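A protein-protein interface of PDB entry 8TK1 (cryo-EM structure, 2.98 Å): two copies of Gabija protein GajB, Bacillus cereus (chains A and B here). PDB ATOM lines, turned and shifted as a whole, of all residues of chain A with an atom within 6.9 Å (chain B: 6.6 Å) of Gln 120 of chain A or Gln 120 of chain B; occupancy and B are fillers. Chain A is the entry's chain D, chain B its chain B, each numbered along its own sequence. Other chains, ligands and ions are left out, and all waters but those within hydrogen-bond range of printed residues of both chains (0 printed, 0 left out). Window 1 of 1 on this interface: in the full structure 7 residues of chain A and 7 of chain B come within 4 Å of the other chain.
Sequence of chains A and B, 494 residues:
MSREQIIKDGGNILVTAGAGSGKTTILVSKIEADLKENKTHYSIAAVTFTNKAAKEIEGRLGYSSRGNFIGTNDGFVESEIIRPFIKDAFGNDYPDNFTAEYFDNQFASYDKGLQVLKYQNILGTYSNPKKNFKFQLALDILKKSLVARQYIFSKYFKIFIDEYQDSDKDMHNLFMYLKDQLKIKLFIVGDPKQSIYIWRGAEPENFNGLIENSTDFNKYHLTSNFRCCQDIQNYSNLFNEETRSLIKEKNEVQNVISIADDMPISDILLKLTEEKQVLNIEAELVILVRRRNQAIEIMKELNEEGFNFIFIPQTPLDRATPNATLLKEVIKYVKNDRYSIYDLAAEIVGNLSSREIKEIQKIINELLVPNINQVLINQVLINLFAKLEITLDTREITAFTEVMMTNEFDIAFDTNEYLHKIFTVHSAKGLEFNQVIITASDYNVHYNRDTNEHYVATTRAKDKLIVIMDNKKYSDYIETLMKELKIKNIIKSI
Asn 105 of chain A touches Gln 120 of chain B (OD1 to N, 3.97 Å). Tyr 119 of chain A touches Ile 122 of chain B. Gln 120 of chain A touches Asn 105 of chain B (N to OD1, 3.8 Å). Asn 121 of chain A touches Ile 122 of chain B (CB to CB, 3.9 Å). Ile 122 of chain A touches Tyr 119 of chain B. CB of Ile 122 of chain A touches CB of Asn 121 of chain B (3.9 Å).
Gln 120 of chain A touches just these residues of chain B: Asn 105, Gln 120, Asn 121 and Ile 122. Gln 120 of chain B touches just these residues of chain A: Asn 105 (3.97 Å), Gln 120 (2.3 Å), Asn 121 (3.3 Å) and Ile 122 (3.0 Å). Of the printed residues of chain B, Ile 122 of chain A touches Tyr 119, Gln 120 and Asn 121. Printed residues of chain A within 4 Å of Asn 121 of chain B: Thr 99 (2.5 Å), Gln 120 (3.4 Å), Asn 121 (3.2 Å) and Ile 122 (3.9 Å). Printed residues of chain A within 4 Å of Ile 122 of chain B: Tyr 119 (3.7 Å), Gln 120 (3.0 Å) and Asn 121 (3.9 Å).
The backbone carbonyl oxygen (O) of Val 116 of chain B is in hydrogen-bond range of the backbone NH (N) of Asn 121 of chain B, 2.9 Å away. The backbone carbonyl oxygen (O) of Val 116 of chain A lies within hydrogen-bond range of the backbone NH (N) of Asn 121 of chain A, 2.8 Å away.
Tyr 119 of chain A touches Ile 122 of chain B, and with the chains exchanged Ile 122 of chain A touches Tyr 119 of chain B. Gln 120 of chain A touches its own counterpart, Gln 120 of chain B. Asn 121 of chain A touches its own counterpart, Asn 121 of chain B. Asn 121 of chain A touches Ile 122 of chain B, and with the chains exchanged Ile 122 of chain A touches Asn 121 of chain B. Positions printed for both chains: 95, 99, 105, 112, 114, 115, 116, 117, 118, 119, 120, 121, 122 and 123.
OD1 of Asn 121 of chain A sits at hydrogen-bond distance from OG1 of Thr 99 of chain B, 2.5 Å away. The side-chain amide oxygen (OD1) of Asn 105 of chain B sits close to the backbone carbonyl oxygen (O) of Tyr 119 of chain A, at 2.9 Å. O of Tyr 119 of chain B sits close to OD1 of Asn 105 of chain A (3.0 Å). O of Gln 120 of chain B sits close to N of Ile 122 of chain A (3.5 Å). OD1 of Asn 121 of chain B lies within hydrogen-bond range of OG1 of Thr 99 of chain A. The backbone carbonyl oxygen (O) of Gln 120 of chain A sits close to the backbone NH (N) of Ile 122 of chain B (3.5 Å). The backbone carbonyl oxygen of Gln 120 of chain A sits close to the backbone carbonyl oxygen of Gln 120 of chain B (2.3 Å). The backbone carbonyl oxygen (O) of Gln 120 of chain A sits close to the backbone carbonyl oxygen (O) of Asn 121 of chain B, at 3.4 Å. The backbone carbonyl oxygen (O) of Asn 121 of chain A lies close to the backbone carbonyl oxygen (O) of Gln 120 of chain B, 3.4 Å away. The backbone carbonyl oxygen of Asn 121 of chain B sits close to the backbone carbonyl oxygen of Asn 121 of chain A (3.2 Å).
Hydrophobic or aromatic side chains of chain B that line the printed part of chain A: Tyr 119 and Ile 122.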
ATOM      1  N   PRO A  95      13.640   6.627  15.699  1.00  0.00           N
ATOM      2  CA  PRO A  95      14.212   6.969  14.395  1.00  0.00           C
ATOM      3  C   PRO A  95      15.354   7.970  14.483  1.00  0.00           C
ATOM      4  O   PRO A  95      15.411   8.828  15.366  1.00  0.00           O
ATOM      5  CB  PRO A  95      13.013   7.582  13.660  1.00  0.00           C
ATOM      6  CG  PRO A  95      12.253   8.274  14.744  1.00  0.00           C
ATOM      7  CD  PRO A  95      12.495   7.497  16.025  1.00  0.00           C
ATOM      8  N   THR A  99      14.131  16.666  10.648  1.00  0.00           N
ATOM      9  CA  THR A  99      14.446  17.901   9.944  1.00  0.00           C
ATOM     10  C   THR A  99      14.340  19.090  10.889  1.00  0.00           C
ATOM     11  O   THR A  99      13.819  20.151  10.530  1.00  0.00           O
ATOM     12  CB  THR A  99      13.531  18.091   8.737  1.00  0.00           C
ATOM     13  OG1 THR A  99      12.179  17.785   9.105  1.00  0.00           O
ATOM     14  CG2 THR A  99      13.961  17.183   7.593  1.00  0.00           C
ATOM     15  N   ASP A 104       6.689  24.970  16.609  1.00  0.00           N
ATOM     16  CA  ASP A 104       5.647  24.414  15.753  1.00  0.00           C
ATOM     17  C   ASP A 104       4.992  23.197  16.405  1.00  0.00           C
ATOM     18  O   ASP A 104       3.768  23.110  16.480  1.00  0.00           O
ATOM     19  CB  ASP A 104       6.224  24.041  14.385  1.00  0.00           C
ATOM     20  CG  ASP A 104       7.431  23.128  14.489  1.00  0.00           C
ATOM     21  OD1 ASP A 104       7.824  22.786  15.624  1.00  0.00           O
ATOM     22  OD2 ASP A 104       7.991  22.759  13.436  1.00  0.00           O
ATOM     23  N   ASN A 105       5.817  22.263  16.880  1.00  0.00           N
ATOM     24  CA  ASN A 105       5.348  21.061  17.559  1.00  0.00           C
ATOM     25  C   ASN A 105       5.891  20.968  18.982  1.00  0.00           C
ATOM     26  O   ASN A 105       5.995  19.875  19.544  1.00  0.00           O
ATOM     27  CB  ASN A 105       5.731  19.817  16.761  1.00  0.00           C
ATOM     28  CG  ASN A 105       4.961  19.693  15.462  1.00  0.00           C
ATOM     29  OD1 ASN A 105       5.549  19.587  14.386  1.00  0.00           O
ATOM     30  ND2 ASN A 105       3.637  19.702  15.554  1.00  0.00           N
ATOM     31  N   LYS A 112       6.711  13.616  25.869  1.00  0.00           N
ATOM     32  CA  LYS A 112       6.115  14.010  24.601  1.00  0.00           C
ATOM     33  C   LYS A 112       7.173  14.297  23.545  1.00  0.00           C
ATOM     34  O   LYS A 112       6.907  14.130  22.355  1.00  0.00           O
ATOM     35  CB  LYS A 112       5.222  15.234  24.787  1.00  0.00           C
ATOM     36  CG  LYS A 112       4.372  15.569  23.566  1.00  0.00           C
ATOM     37  CD  LYS A 112       3.241  14.571  23.380  1.00  0.00           C
ATOM     38  CE  LYS A 112       2.391  14.915  22.169  1.00  0.00           C
ATOM     39  NZ  LYS A 112       1.734  16.244  22.308  1.00  0.00           N
ATOM     40  N   LEU A 114      10.022  12.548  23.118  1.00  0.00           N
ATOM     41  CA  LEU A 114      10.292  11.230  22.554  1.00  0.00           C
ATOM     42  C   LEU A 114       9.121  10.752  21.708  1.00  0.00           C
ATOM     43  O   LEU A 114       9.315  10.143  20.651  1.00  0.00           O
ATOM     44  CB  LEU A 114      10.583  10.224  23.669  1.00  0.00           C
ATOM     45  CG  LEU A 114      11.867  10.432  24.477  1.00  0.00           C
ATOM     46  CD1 LEU A 114      11.598  11.248  25.728  1.00  0.00           C
ATOM     47  CD2 LEU A 114      12.493   9.096  24.840  1.00  0.00           C
ATOM     48  N   GLN A 115       7.895  11.017  22.162  1.00  0.00           N
ATOM     49  CA  GLN A 115       6.724  10.602  21.399  1.00  0.00           C
ATOM     50  C   GLN A 115       6.693  11.275  20.032  1.00  0.00           C
ATOM     51  O   GLN A 115       6.378  10.635  19.023  1.00  0.00           O
ATOM     52  CB  GLN A 115       5.449  10.913  22.180  1.00  0.00           C
ATOM     53  CG  GLN A 115       5.279  10.079  23.439  1.00  0.00           C
ATOM     54  CD  GLN A 115       4.077  10.502  24.259  1.00  0.00           C
ATOM     55  OE1 GLN A 115       3.204  11.222  23.777  1.00  0.00           O
ATOM     56  NE2 GLN A 115       4.026  10.054  25.509  1.00  0.00           N
ATOM     57  N   VAL A 116       7.007  12.570  19.979  1.00  0.00           N
ATOM     58  CA  VAL A 116       7.053  13.275  18.702  1.00  0.00           C
ATOM     59  C   VAL A 116       8.167  12.706  17.832  1.00  0.00           C
ATOM     60  O   VAL A 116       7.955  12.368  16.662  1.00  0.00           O
ATOM     61  CB  VAL A 116       7.228  14.788  18.932  1.00  0.00           C
ATOM     62  CG1 VAL A 116       7.477  15.514  17.617  1.00  0.00           C
ATOM     63  CG2 VAL A 116       6.004  15.363  19.626  1.00  0.00           C
ATOM     64  N   LEU A 117       9.362  12.550  18.404  1.00  0.00           N
ATOM     65  CA  LEU A 117      10.487  12.033  17.630  1.00  0.00           C
ATOM     66  C   LEU A 117      10.174  10.658  17.049  1.00  0.00           C
ATOM     67  O   LEU A 117      10.610  10.334  15.938  1.00  0.00           O
ATOM     68  CB  LEU A 117      11.738  11.974  18.508  1.00  0.00           C
ATOM     69  CG  LEU A 117      13.081  11.725  17.817  1.00  0.00           C
ATOM     70  CD1 LEU A 117      13.312  12.681  16.658  1.00  0.00           C
ATOM     71  CD2 LEU A 117      14.207  11.830  18.829  1.00  0.00           C
ATOM     72  N   LYS A 118       9.420   9.839  17.781  1.00  0.00           N
ATOM     73  CA  LYS A 118       9.141   8.479  17.334  1.00  0.00           C
ATOM     74  C   LYS A 118       7.968   8.434  16.358  1.00  0.00           C
ATOM     75  O   LYS A 118       8.126   8.045  15.196  1.00  0.00           O
ATOM     76  CB  LYS A 118       8.866   7.584  18.545  1.00  0.00           C
ATOM     77  CG  LYS A 118       8.666   6.117  18.205  1.00  0.00           C
ATOM     78  CD  LYS A 118       8.938   5.202  19.397  1.00  0.00           C
ATOM     79  CE  LYS A 118       8.475   5.807  20.717  1.00  0.00           C
ATOM     80  NZ  LYS A 118       8.504   4.814  21.823  1.00  0.00           N
ATOM     81  N   TYR A 119       6.779   8.830  16.818  1.00  0.00           N
ATOM     82  CA  TYR A 119       5.592   8.751  15.973  1.00  0.00           C
ATOM     83  C   TYR A 119       5.636   9.800  14.869  1.00  0.00           C
ATOM     84  O   TYR A 119       5.520   9.472  13.681  1.00  0.00           O
ATOM     85  CB  TYR A 119       4.338   8.934  16.827  1.00  0.00           C
ATOM     86  CG  TYR A 119       4.308   8.073  18.069  1.00  0.00           C
ATOM     87  CD1 TYR A 119       4.468   6.696  17.988  1.00  0.00           C
ATOM     88  CD2 TYR A 119       4.127   8.638  19.322  1.00  0.00           C
ATOM     89  CE1 TYR A 119       4.443   5.908  19.122  1.00  0.00           C
ATOM     90  CE2 TYR A 119       4.100   7.859  20.461  1.00  0.00           C
ATOM     91  CZ  TYR A 119       4.259   6.495  20.356  1.00  0.00           C
ATOM     92  OH  TYR A 119       4.233   5.716  21.491  1.00  0.00           O
ATOM     93  N   GLN A 120       5.802  11.069  15.244  1.00  0.00           N
ATOM     94  CA  GLN A 120       5.783  12.142  14.261  1.00  0.00           C
ATOM     95  C   GLN A 120       7.034  12.133  13.395  1.00  0.00           C
ATOM     96  O   GLN A 120       6.980  12.546  12.233  1.00  0.00           O
ATOM     97  CB  GLN A 120       5.631  13.485  14.974  1.00  0.00           C
ATOM     98  CG  GLN A 120       4.393  13.574  15.856  1.00  0.00           C
ATOM     99  CD  GLN A 120       3.977  15.002  16.152  1.00  0.00           C
ATOM    100  OE1 GLN A 120       4.524  15.950  15.591  1.00  0.00           O
ATOM    101  NE2 GLN A 120       3.005  15.161  17.040  1.00  0.00           N
ATOM    102  N   ASN A 121       8.160  11.656  13.928  1.00  0.00           N
ATOM    103  CA  ASN A 121       9.420  11.586  13.186  1.00  0.00           C
ATOM    104  C   ASN A 121       9.972  12.986  12.915  1.00  0.00           C
ATOM    105  O   ASN A 121      10.405  13.308  11.808  1.00  0.00           O
ATOM    106  CB  ASN A 121       9.242  10.801  11.883  1.00  0.00           C
ATOM    107  CG  ASN A 121      10.556  10.522  11.182  1.00  0.00           C
ATOM    108  OD1 ASN A 121      10.591   9.878  10.135  1.00  0.00           O
ATOM    109  ND2 ASN A 121      11.648  11.009  11.758  1.00  0.00           N
ATOM    110  N   ILE A 122       9.952  13.823  13.950  1.00  0.00           N
ATOM    111  CA  ILE A 122      10.523  15.166  13.891  1.00  0.00           C
ATOM    112  C   ILE A 122      11.073  15.497  15.269  1.00  0.00           C
ATOM    113  O   ILE A 122      10.505  15.097  16.290  1.00  0.00           O
ATOM    114  CB  ILE A 122       9.484  16.210  13.424  1.00  0.00           C
ATOM    115  CG1 ILE A 122      10.105  17.607  13.330  1.00  0.00           C
ATOM    116  CG2 ILE A 122       8.283  16.228  14.359  1.00  0.00           C
ATOM    117  CD1 ILE A 122      11.011  17.787  12.137  1.00  0.00           C
ATOM    118  N   LEU A 123      12.183  16.227  15.299  1.00  0.00           N
ATOM    119  CA  LEU A 123      12.820  16.547  16.568  1.00  0.00           C
ATOM    120  C   LEU A 123      11.908  17.429  17.412  1.00  0.00           C
ATOM    121  O   LEU A 123      11.288  18.373  16.911  1.00  0.00           O
ATOM    122  CB  LEU A 123      14.158  17.248  16.326  1.00  0.00           C
ATOM    123  CG  LEU A 123      15.192  17.091  17.442  1.00  0.00           C
ATOM    124  CD1 LEU A 123      15.720  15.665  17.491  1.00  0.00           C
ATOM    125  CD2 LEU A 123      16.332  18.076  17.255  1.00  0.00           C
ATOM    126  N   PRO B  95       8.518  18.612   3.204  1.00  0.00           N
ATOM    127  CA  PRO B  95       9.720  17.786   3.329  1.00  0.00           C
ATOM    128  C   PRO B  95       9.659  16.504   2.515  1.00  0.00           C
ATOM    129  O   PRO B  95       8.602  15.913   2.295  1.00  0.00           O
ATOM    130  CB  PRO B  95       9.749  17.470   4.829  1.00  0.00           C
ATOM    131  CG  PRO B  95       8.306  17.371   5.194  1.00  0.00           C
ATOM    132  CD  PRO B  95       7.545  18.306   4.270  1.00  0.00           C
ATOM    133  N   THR B  99       9.556   8.173   7.211  1.00  0.00           N
ATOM    134  CA  THR B  99       9.835   6.779   7.524  1.00  0.00           C
ATOM    135  C   THR B  99       8.550   5.966   7.516  1.00  0.00           C
ATOM    136  O   THR B  99       8.324   5.111   8.377  1.00  0.00           O
ATOM    137  CB  THR B  99      10.541   6.653   8.871  1.00  0.00           C
ATOM    138  OG1 THR B  99       9.893   7.494   9.835  1.00  0.00           O
ATOM    139  CG2 THR B  99      12.003   7.056   8.751  1.00  0.00           C
ATOM    140  N   ASN B 105      -0.363   7.383  13.267  1.00  0.00           N
ATOM    141  CA  ASN B 105      -0.677   8.794  13.077  1.00  0.00           C
ATOM    142  C   ASN B 105      -1.679   8.989  11.942  1.00  0.00           C
ATOM    143  O   ASN B 105      -1.603   9.968  11.199  1.00  0.00           O
ATOM    144  CB  ASN B 105       0.594   9.600  12.811  1.00  0.00           C
ATOM    145  CG  ASN B 105       1.460   9.749  14.046  1.00  0.00           C
ATOM    146  OD1 ASN B 105       2.643   9.407  14.032  1.00  0.00           O
ATOM    147  ND2 ASN B 105       0.878  10.265  15.121  1.00  0.00           N
ATOM    148  N   PHE B 107      -5.308   9.781  10.146  1.00  0.00           N
ATOM    149  CA  PHE B 107      -6.365  10.764  10.355  1.00  0.00           C
ATOM    150  C   PHE B 107      -7.467  10.493   9.335  1.00  0.00           C
ATOM    151  O   PHE B 107      -7.476   9.457   8.663  1.00  0.00           O
ATOM    152  CB  PHE B 107      -5.813  12.193  10.258  1.00  0.00           C
ATOM    153  CG  PHE B 107      -4.875  12.559  11.375  1.00  0.00           C
ATOM    154  CD1 PHE B 107      -3.559  12.132  11.365  1.00  0.00           C
ATOM    155  CD2 PHE B 107      -5.315  13.326  12.441  1.00  0.00           C
ATOM    156  CE1 PHE B 107      -2.697  12.468  12.390  1.00  0.00           C
ATOM    157  CE2 PHE B 107      -4.455  13.664  13.470  1.00  0.00           C
ATOM    158  CZ  PHE B 107      -3.146  13.233  13.443  1.00  0.00           C
ATOM    159  N   LYS B 112      -5.151  17.335   6.783  1.00  0.00           N
ATOM    160  CA  LYS B 112      -4.399  16.911   7.956  1.00  0.00           C
ATOM    161  C   LYS B 112      -3.277  15.954   7.584  1.00  0.00           C
ATOM    162  O   LYS B 112      -2.257  15.911   8.274  1.00  0.00           O
ATOM    163  CB  LYS B 112      -5.330  16.260   8.981  1.00  0.00           C
ATOM    164  CG  LYS B 112      -4.691  16.032  10.346  1.00  0.00           C
ATOM    165  CD  LYS B 112      -4.285  17.340  11.011  1.00  0.00           C
ATOM    166  CE  LYS B 112      -3.769  17.116  12.421  1.00  0.00           C
ATOM    167  NZ  LYS B 112      -4.866  16.765  13.364  1.00  0.00           N
ATOM    168  N   LEU B 114      -1.445  16.309   4.805  1.00  0.00           N
ATOM    169  CA  LEU B 114      -0.389  17.251   4.439  1.00  0.00           C
ATOM    170  C   LEU B 114       0.229  17.881   5.678  1.00  0.00           C
ATOM    171  O   LEU B 114       1.450  18.063   5.752  1.00  0.00           O
ATOM    172  CB  LEU B 114      -0.936  18.342   3.517  1.00  0.00           C
ATOM    173  CG  LEU B 114      -1.155  17.999   2.044  1.00  0.00           C
ATOM    174  CD1 LEU B 114      -2.369  17.122   1.871  1.00  0.00           C
ATOM    175  CD2 LEU B 114      -1.292  19.264   1.212  1.00  0.00           C
ATOM    176  N   GLN B 115      -0.603  18.233   6.658  1.00  0.00           N
ATOM    177  CA  GLN B 115      -0.095  18.847   7.879  1.00  0.00           C
ATOM    178  C   GLN B 115       0.830  17.897   8.628  1.00  0.00           C
ATOM    179  O   GLN B 115       1.859  18.316   9.163  1.00  0.00           O
ATOM    180  CB  GLN B 115      -1.259  19.278   8.771  1.00  0.00           C
ATOM    181  CG  GLN B 115      -2.077  20.422   8.199  1.00  0.00           C
ATOM    182  CD  GLN B 115      -3.342  20.688   8.993  1.00  0.00           C
ATOM    183  OE1 GLN B 115      -3.472  20.256  10.138  1.00  0.00           O
ATOM    184  NE2 GLN B 115      -4.284  21.399   8.385  1.00  0.00           N
ATOM    185  N   VAL B 116       0.474  16.614   8.690  1.00  0.00           N
ATOM    186  CA  VAL B 116       1.353  15.632   9.319  1.00  0.00           C
ATOM    187  C   VAL B 116       2.664  15.538   8.551  1.00  0.00           C
ATOM    188  O   VAL B 116       3.750  15.651   9.127  1.00  0.00           O
ATOM    189  CB  VAL B 116       0.650  14.264   9.414  1.00  0.00           C
ATOM    190  CG1 VAL B 116       1.628  13.186   9.857  1.00  0.00           C
ATOM    191  CG2 VAL B 116      -0.526  14.338  10.373  1.00  0.00           C
ATOM    192  N   LEU B 117       2.580  15.380   7.229  1.00  0.00           N
ATOM    193  CA  LEU B 117       3.795  15.263   6.428  1.00  0.00           C
ATOM    194  C   LEU B 117       4.710  16.468   6.625  1.00  0.00           C
ATOM    195  O   LEU B 117       5.938  16.326   6.643  1.00  0.00           O
ATOM    196  CB  LEU B 117       3.434  15.099   4.951  1.00  0.00           C
ATOM    197  CG  LEU B 117       4.572  14.736   3.991  1.00  0.00           C
ATOM    198  CD1 LEU B 117       5.372  13.539   4.482  1.00  0.00           C
ATOM    199  CD2 LEU B 117       4.012  14.470   2.606  1.00  0.00           C
ATOM    200  N   LYS B 118       4.133  17.659   6.776  1.00  0.00           N
ATOM    201  CA  LYS B 118       4.944  18.871   6.877  1.00  0.00           C
ATOM    202  C   LYS B 118       5.455  19.094   8.297  1.00  0.00           C
ATOM    203  O   LYS B 118       6.664  19.065   8.545  1.00  0.00           O
ATOM    204  CB  LYS B 118       4.130  20.078   6.404  1.00  0.00           C
ATOM    205  CG  LYS B 118       4.910  21.382   6.387  1.00  0.00           C
ATOM    206  CD  LYS B 118       4.297  22.414   5.446  1.00  0.00           C
ATOM    207  CE  LYS B 118       2.774  22.382   5.454  1.00  0.00           C
ATOM    208  NZ  LYS B 118       2.187  23.546   4.737  1.00  0.00           N
ATOM    209  N   TYR B 119       4.542  19.321   9.242  1.00  0.00           N
ATOM    210  CA  TYR B 119       4.947  19.631  10.609  1.00  0.00           C
ATOM    211  C   TYR B 119       5.570  18.418  11.287  1.00  0.00           C
ATOM    212  O   TYR B 119       6.661  18.506  11.864  1.00  0.00           O
ATOM    213  CB  TYR B 119       3.737  20.118  11.408  1.00  0.00           C
ATOM    214  CG  TYR B 119       2.946  21.209  10.723  1.00  0.00           C
ATOM    215  CD1 TYR B 119       3.562  22.377  10.294  1.00  0.00           C
ATOM    216  CD2 TYR B 119       1.585  21.065  10.498  1.00  0.00           C
ATOM    217  CE1 TYR B 119       2.840  23.373   9.667  1.00  0.00           C
ATOM    218  CE2 TYR B 119       0.855  22.055   9.872  1.00  0.00           C
ATOM    219  CZ  TYR B 119       1.486  23.207   9.458  1.00  0.00           C
ATOM    220  OH  TYR B 119       0.763  24.196   8.832  1.00  0.00           O
ATOM    221  N   GLN B 120       4.888  17.273  11.228  1.00  0.00           N
ATOM    222  CA  GLN B 120       5.368  16.087  11.926  1.00  0.00           C
ATOM    223  C   GLN B 120       6.534  15.438  11.195  1.00  0.00           C
ATOM    224  O   GLN B 120       7.386  14.813  11.830  1.00  0.00           O
ATOM    225  CB  GLN B 120       4.220  15.094  12.100  1.00  0.00           C
ATOM    226  CG  GLN B 120       3.027  15.664  12.855  1.00  0.00           C
ATOM    227  CD  GLN B 120       2.131  14.592  13.443  1.00  0.00           C
ATOM    228  OE1 GLN B 120       2.457  13.407  13.412  1.00  0.00           O
ATOM    229  NE2 GLN B 120       0.991  15.007  13.982  1.00  0.00           N
ATOM    230  N   ASN B 121       6.600  15.585   9.871  1.00  0.00           N
ATOM    231  CA  ASN B 121       7.677  15.016   9.063  1.00  0.00           C
ATOM    232  C   ASN B 121       7.590  13.487   9.036  1.00  0.00           C
ATOM    233  O   ASN B 121       8.581  12.772   9.192  1.00  0.00           O
ATOM    234  CB  ASN B 121       9.044  15.485   9.577  1.00  0.00           C
ATOM    235  CG  ASN B 121      10.181  15.097   8.655  1.00  0.00           C
ATOM    236  OD1 ASN B 121      11.340  15.422   8.910  1.00  0.00           O
ATOM    237  ND2 ASN B 121       9.856  14.402   7.572  1.00  0.00           N
ATOM    238  N   ILE B 122       6.369  12.998   8.832  1.00  0.00           N
ATOM    239  CA  ILE B 122       6.104  11.569   8.688  1.00  0.00           C
ATOM    240  C   ILE B 122       4.942  11.404   7.721  1.00  0.00           C
ATOM    241  O   ILE B 122       4.005  12.206   7.716  1.00  0.00           O
ATOM    242  CB  ILE B 122       5.807  10.903  10.050  1.00  0.00           C
ATOM    243  CG1 ILE B 122       5.586   9.397   9.889  1.00  0.00           C
ATOM    244  CG2 ILE B 122       4.602  11.551  10.717  1.00  0.00           C
ATOM    245  CD1 ILE B 122       6.855   8.619   9.650  1.00  0.00           C
ATOM    246  N   LEU B 123       5.008  10.360   6.898  1.00  0.00           N
ATOM    247  CA  LEU B 123       3.972  10.141   5.899  1.00  0.00           C
ATOM    248  C   LEU B 123       2.629   9.871   6.568  1.00  0.00           C
ATOM    249  O   LEU B 123       2.544   9.138   7.556  1.00  0.00           O
ATOM    250  CB  LEU B 123       4.358   8.975   4.989  1.00  0.00           C
ATOM    251  CG  LEU B 123       3.757   9.025   3.583  1.00  0.00           C
ATOM    252  CD1 LEU B 123       4.387  10.140   2.761  1.00  0.00           C
ATOM    253  CD2 LEU B 123       3.925   7.692   2.888  1.00  0.00           C
